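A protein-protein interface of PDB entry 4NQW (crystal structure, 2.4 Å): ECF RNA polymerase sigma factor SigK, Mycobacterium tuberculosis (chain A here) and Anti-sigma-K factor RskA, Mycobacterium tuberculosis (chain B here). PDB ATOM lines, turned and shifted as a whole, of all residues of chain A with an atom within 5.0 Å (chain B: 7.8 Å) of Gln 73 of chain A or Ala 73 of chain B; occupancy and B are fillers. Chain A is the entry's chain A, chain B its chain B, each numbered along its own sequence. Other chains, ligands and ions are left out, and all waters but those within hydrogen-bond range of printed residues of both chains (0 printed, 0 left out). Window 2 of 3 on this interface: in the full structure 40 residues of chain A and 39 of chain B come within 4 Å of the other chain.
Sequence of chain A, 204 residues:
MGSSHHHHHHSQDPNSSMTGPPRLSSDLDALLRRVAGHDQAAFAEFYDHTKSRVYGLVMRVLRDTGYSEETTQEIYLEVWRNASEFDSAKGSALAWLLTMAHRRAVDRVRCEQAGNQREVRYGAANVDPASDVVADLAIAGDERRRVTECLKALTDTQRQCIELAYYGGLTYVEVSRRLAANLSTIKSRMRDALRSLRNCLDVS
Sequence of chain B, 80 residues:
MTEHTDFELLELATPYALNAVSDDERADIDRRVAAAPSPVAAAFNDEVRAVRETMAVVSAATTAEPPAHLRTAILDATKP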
ATOM      1  N   GLU A  69       0.946 -23.622  23.517  1.00  0.00           N
ATOM      2  CA  GLU A  69      -0.478 -23.941  23.527  1.00  0.00           C
ATOM      3  C   GLU A  69      -1.047 -23.953  22.108  1.00  0.00           C
ATOM      4  O   GLU A  69      -1.714 -24.906  21.709  1.00  0.00           O
ATOM      5  CB  GLU A  69      -1.250 -22.942  24.397  1.00  0.00           C
ATOM      6  CG  GLU A  69      -0.980 -23.089  25.886  1.00  0.00           C
ATOM      7  CD  GLU A  69      -1.658 -22.021  26.732  1.00  0.00           C
ATOM      8  OE1 GLU A  69      -2.438 -21.207  26.189  1.00  0.00           O
ATOM      9  OE2 GLU A  69      -1.412 -21.992  27.957  1.00  0.00           O
ATOM     10  N   GLU A  70      -0.768 -22.900  21.347  1.00  0.00           N
ATOM     11  CA  GLU A  70      -1.268 -22.793  19.973  1.00  0.00           C
ATOM     12  C   GLU A  70      -0.723 -23.894  19.062  1.00  0.00           C
ATOM     13  O   GLU A  70      -1.456 -24.445  18.243  1.00  0.00           O
ATOM     14  CB  GLU A  70      -0.941 -21.420  19.386  1.00  0.00           C
ATOM     15  CG  GLU A  70      -1.685 -20.284  20.070  1.00  0.00           C
ATOM     16  CD  GLU A  70      -1.449 -18.936  19.417  1.00  0.00           C
ATOM     17  OE1 GLU A  70      -0.643 -18.853  18.466  1.00  0.00           O
ATOM     18  OE2 GLU A  70      -2.077 -17.956  19.861  1.00  0.00           O
ATOM     19  N   THR A  71       0.561 -24.207  19.209  1.00  0.00           N
ATOM     20  CA  THR A  71       1.190 -25.278  18.437  1.00  0.00           C
ATOM     21  C   THR A  71       0.568 -26.635  18.773  1.00  0.00           C
ATOM     22  O   THR A  71       0.312 -27.437  17.877  1.00  0.00           O
ATOM     23  CB  THR A  71       2.708 -25.327  18.688  1.00  0.00           C
ATOM     24  OG1 THR A  71       3.278 -24.040  18.426  1.00  0.00           O
ATOM     25  CG2 THR A  71       3.382 -26.371  17.803  1.00  0.00           C
ATOM     26  N   THR A  72       0.321 -26.881  20.057  1.00  0.00           N
ATOM     27  CA  THR A  72      -0.316 -28.124  20.501  1.00  0.00           C
ATOM     28  C   THR A  72      -1.711 -28.294  19.890  1.00  0.00           C
ATOM     29  O   THR A  72      -2.086 -29.401  19.507  1.00  0.00           O
ATOM     30  CB  THR A  72      -0.384 -28.208  22.042  1.00  0.00           C
ATOM     31  OG1 THR A  72       0.944 -28.186  22.580  1.00  0.00           O
ATOM     32  CG2 THR A  72      -1.075 -29.488  22.497  1.00  0.00           C
ATOM     33  N   GLN A  73      -2.465 -27.199  19.793  1.00  0.00           N
ATOM     34  CA  GLN A  73      -3.771 -27.208  19.123  1.00  0.00           C
ATOM     35  C   GLN A  73      -3.645 -27.594  17.657  1.00  0.00           C
ATOM     36  O   GLN A  73      -4.404 -28.428  17.163  1.00  0.00           O
ATOM     37  CB  GLN A  73      -4.437 -25.834  19.193  1.00  0.00           C
ATOM     38  CG  GLN A  73      -5.015 -25.472  20.542  1.00  0.00           C
ATOM     39  CD  GLN A  73      -5.726 -24.132  20.506  1.00  0.00           C
ATOM     40  OE1 GLN A  73      -5.142 -23.120  20.117  1.00  0.00           O
ATOM     41  NE2 GLN A  73      -6.990 -24.119  20.901  1.00  0.00           N
ATOM     42  N   GLU A  74      -2.700 -26.962  16.965  1.00  0.00           N
ATOM     43  CA  GLU A  74      -2.444 -27.260  15.559  1.00  0.00           C
ATOM     44  C   GLU A  74      -2.123 -28.740  15.374  1.00  0.00           C
ATOM     45  O   GLU A  74      -2.576 -29.360  14.415  1.00  0.00           O
ATOM     46  CB  GLU A  74      -1.291 -26.407  15.022  1.00  0.00           C
ATOM     47  CG  GLU A  74      -1.627 -24.934  14.839  1.00  0.00           C
ATOM     48  CD  GLU A  74      -0.431 -24.094  14.414  1.00  0.00           C
ATOM     49  OE1 GLU A  74       0.659 -24.657  14.167  1.00  0.00           O
ATOM     50  OE2 GLU A  74      -0.583 -22.858  14.327  1.00  0.00           O
ATOM     51  N   ILE A  75      -1.350 -29.296  16.307  1.00  0.00           N
ATOM     52  CA  ILE A  75      -0.935 -30.698  16.248  1.00  0.00           C
ATOM     53  C   ILE A  75      -2.140 -31.631  16.322  1.00  0.00           C
ATOM     54  O   ILE A  75      -2.288 -32.514  15.483  1.00  0.00           O
ATOM     55  CB  ILE A  75       0.080 -31.042  17.363  1.00  0.00           C
ATOM     56  CG1 ILE A  75       1.401 -30.312  17.105  1.00  0.00           C
ATOM     57  CG2 ILE A  75       0.342 -32.541  17.417  1.00  0.00           C
ATOM     58  CD1 ILE A  75       2.311 -30.186  18.311  1.00  0.00           C
ATOM     59  N   TYR A  76      -3.007 -31.424  17.309  1.00  0.00           N
ATOM     60  CA  TYR A  76      -4.194 -32.270  17.468  1.00  0.00           C
ATOM     61  C   TYR A  76      -5.275 -32.005  16.416  1.00  0.00           C
ATOM     62  O   TYR A  76      -6.101 -32.883  16.149  1.00  0.00           O
ATOM     63  CB  TYR A  76      -4.758 -32.164  18.889  1.00  0.00           C
ATOM     64  CG  TYR A  76      -3.905 -32.909  19.886  1.00  0.00           C
ATOM     65  CD1 TYR A  76      -3.037 -32.233  20.738  1.00  0.00           C
ATOM     66  CD2 TYR A  76      -3.941 -34.296  19.953  1.00  0.00           C
ATOM     67  CE1 TYR A  76      -2.240 -32.920  21.641  1.00  0.00           C
ATOM     68  CE2 TYR A  76      -3.149 -34.991  20.850  1.00  0.00           C
ATOM     69  CZ  TYR A  76      -2.302 -34.299  21.691  1.00  0.00           C
ATOM     70  OH  TYR A  76      -1.520 -34.991  22.585  1.00  0.00           O
ATOM     71  N   LEU A  77      -5.266 -30.819  15.809  1.00  0.00           N
ATOM     72  CA  LEU A  77      -6.116 -30.565  14.641  1.00  0.00           C
ATOM     73  C   LEU A  77      -5.625 -31.415  13.466  1.00  0.00           C
ATOM     74  O   LEU A  77      -6.432 -32.007  12.756  1.00  0.00           O
ATOM     75  CB  LEU A  77      -6.137 -29.072  14.272  1.00  0.00           C
ATOM     76  CG  LEU A  77      -7.186 -28.542  13.273  1.00  0.00           C
ATOM     77  CD1 LEU A  77      -6.910 -28.975  11.836  1.00  0.00           C
ATOM     78  CD2 LEU A  77      -8.607 -28.922  13.672  1.00  0.00           C
ATOM     79  N   GLU A  78      -4.306 -31.490  13.272  1.00  0.00           N
ATOM     80  CA  GLU A  78      -3.743 -32.357  12.227  1.00  0.00           C
ATOM     81  C   GLU A  78      -3.996 -33.836  12.522  1.00  0.00           C
ATOM     82  O   GLU A  78      -4.252 -34.609  11.600  1.00  0.00           O
ATOM     83  CB  GLU A  78      -2.241 -32.117  12.018  1.00  0.00           C
ATOM     84  CG  GLU A  78      -1.661 -32.968  10.887  1.00  0.00           C
ATOM     85  CD  GLU A  78      -0.212 -32.665  10.550  1.00  0.00           C
ATOM     86  OE1 GLU A  78       0.356 -33.391   9.707  1.00  0.00           O
ATOM     87  OE2 GLU A  78       0.367 -31.714  11.113  1.00  0.00           O
ATOM     88  N   ALA B  68      -6.088 -26.922  31.399  1.00  0.00           N
ATOM     89  CA  ALA B  68      -7.373 -27.551  31.100  1.00  0.00           C
ATOM     90  C   ALA B  68      -8.138 -26.860  29.964  1.00  0.00           C
ATOM     91  O   ALA B  68      -8.932 -27.504  29.279  1.00  0.00           O
ATOM     92  CB  ALA B  68      -8.236 -27.607  32.354  1.00  0.00           C
ATOM     93  N   HIS B  69      -7.901 -25.564  29.762  1.00  0.00           N
ATOM     94  CA  HIS B  69      -8.615 -24.812  28.722  1.00  0.00           C
ATOM     95  C   HIS B  69      -8.255 -25.275  27.307  1.00  0.00           C
ATOM     96  O   HIS B  69      -9.035 -25.092  26.373  1.00  0.00           O
ATOM     97  CB  HIS B  69      -8.385 -23.297  28.872  1.00  0.00           C
ATOM     98  CG  HIS B  69      -7.068 -22.818  28.340  1.00  0.00           C
ATOM     99  ND1 HIS B  69      -6.816 -22.681  26.990  1.00  0.00           N
ATOM    100  CD2 HIS B  69      -5.944 -22.409  28.975  1.00  0.00           C
ATOM    101  CE1 HIS B  69      -5.587 -22.232  26.818  1.00  0.00           C
ATOM    102  NE2 HIS B  69      -5.038 -22.056  28.006  1.00  0.00           N
ATOM    103  N   LEU B  70      -7.074 -25.865  27.150  1.00  0.00           N
ATOM    104  CA  LEU B  70      -6.622 -26.328  25.843  1.00  0.00           C
ATOM    105  C   LEU B  70      -7.429 -27.541  25.384  1.00  0.00           C
ATOM    106  O   LEU B  70      -7.753 -27.665  24.204  1.00  0.00           O
ATOM    107  CB  LEU B  70      -5.124 -26.654  25.879  1.00  0.00           C
ATOM    108  CG  LEU B  70      -4.377 -26.540  24.553  1.00  0.00           C
ATOM    109  CD1 LEU B  70      -4.590 -25.169  23.926  1.00  0.00           C
ATOM    110  CD2 LEU B  70      -2.897 -26.803  24.773  1.00  0.00           C
ATOM    111  N   ARG B  71      -7.756 -28.424  26.325  1.00  0.00           N
ATOM    112  CA  ARG B  71      -8.624 -29.571  26.053  1.00  0.00           C
ATOM    113  C   ARG B  71      -9.961 -29.118  25.465  1.00  0.00           C
ATOM    114  O   ARG B  71     -10.421 -29.670  24.467  1.00  0.00           O
ATOM    115  CB  ARG B  71      -8.865 -30.374  27.334  1.00  0.00           C
ATOM    116  CG  ARG B  71      -9.686 -31.642  27.140  1.00  0.00           C
ATOM    117  CD  ARG B  71      -9.770 -32.460  28.421  1.00  0.00           C
ATOM    118  NE  ARG B  71     -11.041 -33.179  28.531  1.00  0.00           N
ATOM    119  CZ  ARG B  71     -11.321 -34.346  27.948  1.00  0.00           C
ATOM    120  NH1 ARG B  71     -10.427 -34.967  27.185  1.00  0.00           N
ATOM    121  NH2 ARG B  71     -12.517 -34.896  28.126  1.00  0.00           N
ATOM    122  N   THR B  72     -10.568 -28.110  26.086  1.00  0.00           N
ATOM    123  CA  THR B  72     -11.856 -27.568  25.639  1.00  0.00           C
ATOM    124  C   THR B  72     -11.818 -27.132  24.173  1.00  0.00           C
ATOM    125  O   THR B  72     -12.687 -27.508  23.386  1.00  0.00           O
ATOM    126  CB  THR B  72     -12.293 -26.373  26.517  1.00  0.00           C
ATOM    127  OG1 THR B  72     -12.607 -26.840  27.833  1.00  0.00           O
ATOM    128  CG2 THR B  72     -13.513 -25.663  25.935  1.00  0.00           C
ATOM    129  N   ALA B  73     -10.809 -26.345  23.815  1.00  0.00           N
ATOM    130  CA  ALA B  73     -10.689 -25.825  22.452  1.00  0.00           C
ATOM    131  C   ALA B  73     -10.323 -26.913  21.436  1.00  0.00           C
ATOM    132  O   ALA B  73     -10.758 -26.858  20.284  1.00  0.00           O
ATOM    133  CB  ALA B  73      -9.678 -24.691  22.410  1.00  0.00           C
ATOM    134  N   ILE B  74      -9.530 -27.895  21.862  1.00  0.00           N
ATOM    135  CA  ILE B  74      -9.112 -28.994  20.982  1.00  0.00           C
ATOM    136  C   ILE B  74     -10.284 -29.912  20.625  1.00  0.00           C
ATOM    137  O   ILE B  74     -10.488 -30.232  19.452  1.00  0.00           O
ATOM    138  CB  ILE B  74      -7.953 -29.814  21.603  1.00  0.00           C
ATOM    139  CG1 ILE B  74      -6.639 -29.041  21.448  1.00  0.00           C
ATOM    140  CG2 ILE B  74      -7.817 -31.178  20.933  1.00  0.00           C
ATOM    141  CD1 ILE B  74      -5.464 -29.635  22.197  1.00  0.00           C
ATOM    142  N   LEU B  75     -11.046 -30.336  21.629  1.00  0.00           N
ATOM    143  CA  LEU B  75     -12.194 -31.216  21.389  1.00  0.00           C
ATOM    144  C   LEU B  75     -13.304 -30.498  20.624  1.00  0.00           C
ATOM    145  O   LEU B  75     -14.062 -31.137  19.892  1.00  0.00           O
ATOM    146  CB  LEU B  75     -12.747 -31.778  22.704  1.00  0.00           C
ATOM    147  CG  LEU B  75     -11.775 -32.525  23.626  1.00  0.00           C
ATOM    148  CD1 LEU B  75     -12.548 -33.277  24.703  1.00  0.00           C
ATOM    149  CD2 LEU B  75     -10.867 -33.477  22.861  1.00  0.00           C
ATOM    150  N   ASP B  76     -13.391 -29.179  20.787  1.00  0.00           N
ATOM    151  CA  ASP B  76     -14.412 -28.381  20.107  1.00  0.00           C
ATOM    152  C   ASP B  76     -14.081 -28.131  18.638  1.00  0.00           C
ATOM    153  O   ASP B  76     -14.986 -27.966  17.819  1.00  0.00           O
ATOM    154  CB  ASP B  76     -14.610 -27.038  20.810  1.00  0.00           C
ATOM    155  CG  ASP B  76     -15.863 -26.325  20.348  1.00  0.00           C
ATOM    156  OD1 ASP B  76     -15.767 -25.157  19.917  1.00  0.00           O
ATOM    157  OD2 ASP B  76     -16.952 -26.933  20.398  1.00  0.00           O
ATOM    158  N   ALA B  77     -12.792 -28.104  18.308  1.00  0.00           N
ATOM    159  CA  ALA B  77     -12.342 -27.836  16.938  1.00  0.00           C
ATOM    160  C   ALA B  77     -12.740 -28.930  15.939  1.00  0.00           C
ATOM    161  O   ALA B  77     -12.627 -28.735  14.729  1.00  0.00           O
ATOM    162  CB  ALA B  77     -10.834 -27.622  16.911  1.00  0.00           C
ATOM    163  N   THR B  78     -13.209 -30.068  16.447  1.00  0.00           N
ATOM    164  CA  THR B  78     -13.687 -31.167  15.603  1.00  0.00           C
ATOM    165  C   THR B  78     -15.014 -30.863  14.890  1.00  0.00           C
ATOM    166  O   THR B  78     -15.383 -31.559  13.942  1.00  0.00           O
ATOM    167  CB  THR B  78     -13.875 -32.455  16.433  1.00  0.00           C
ATOM    168  OG1 THR B  78     -14.834 -32.227  17.474  1.00  0.00           O
ATOM    169  CG2 THR B  78     -12.555 -32.897  17.050  1.00  0.00           C
ATOM    170  N   LYS B  79     -15.720 -29.829  15.345  1.00  0.00           N
ATOM    171  CA  LYS B  79     -17.059 -29.510  14.851  1.00  0.00           C
ATOM    172  C   LYS B  79     -17.033 -28.276  13.955  1.00  0.00           C
ATOM    173  O   LYS B  79     -16.231 -27.362  14.159  1.00  0.00           O
ATOM    174  CB  LYS B  79     -18.006 -29.278  16.034  1.00  0.00           C
ATOM    175  CG  LYS B  79     -17.868 -30.312  17.144  1.00  0.00           C
ATOM    176  CD  LYS B  79     -18.652 -29.928  18.386  1.00  0.00           C
ATOM    177  CE  LYS B  79     -18.292 -30.836  19.551  1.00  0.00           C
ATOM    178  NZ  LYS B  79     -19.125 -30.576  20.759  1.00  0.00           N
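Of the printed residues of chain B, Thr 72 of chain A touches Leu 70.
Gln 73 of chain A touches just these residues of chain B: Leu 70 and Ala 73.
Printed residues of chain B within 4 Å of Tyr 76 of chain A: Ile 74 (3.8 Å).
Of the printed residues of chain A, Leu 70 of chain B touches Glu 69 (3.6 Å), Thr 72 (3.96 Å) and Gln 73 (3.4 Å).
Ala 73 of chain B touches one residue of chain A.
Of the printed residues of chain A, Ile 74 of chain B touches Tyr 76.
The nearest residue of chain B that does not touch Gln 73 of chain A is Ile 74 of chain B (4.02 Å).
The nearest printed residue of chain A that does not touch Ala 73 of chain B is Leu 77 of chain A (7.3 Å).
Of the 10 printed residues of chain A, 4 touch a printed residue of chain B.
Of the 12 printed residues of chain B, 4 touch a printed residue of chain A.
Hydrophobic or aromatic side chains of chain B within 4 Å of the printed part of chain A: His 69, Leu 70, Ala 73 and Ile 74.
Among the printed residues, no Asp or Glu carboxylate lies within 4 Å of a Lys or Arg side-chain nitrogen of the other chain.
CD1 of Leu 70 of chain B touches O of Glu 69 of chain A (3.6 Å).
CG2 of Thr 72 of chain A touches CD2 of Leu 70 of chain B (3.96 Å).
Gln 73 of chain A touches Leu 70 of chain B.
CB of Ala 73 of chain B touches NE2 of Gln 73 of chain A, 3.1 Å away.
CG2 of Ile 74 of chain B touches CB of Tyr 76 of chain A, at 3.8 Å.
A ring nitrogen (NE2) of His 69 of chain B lies close to the side-chain carboxylate of Glu 69 of chain A (3.3 Å).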
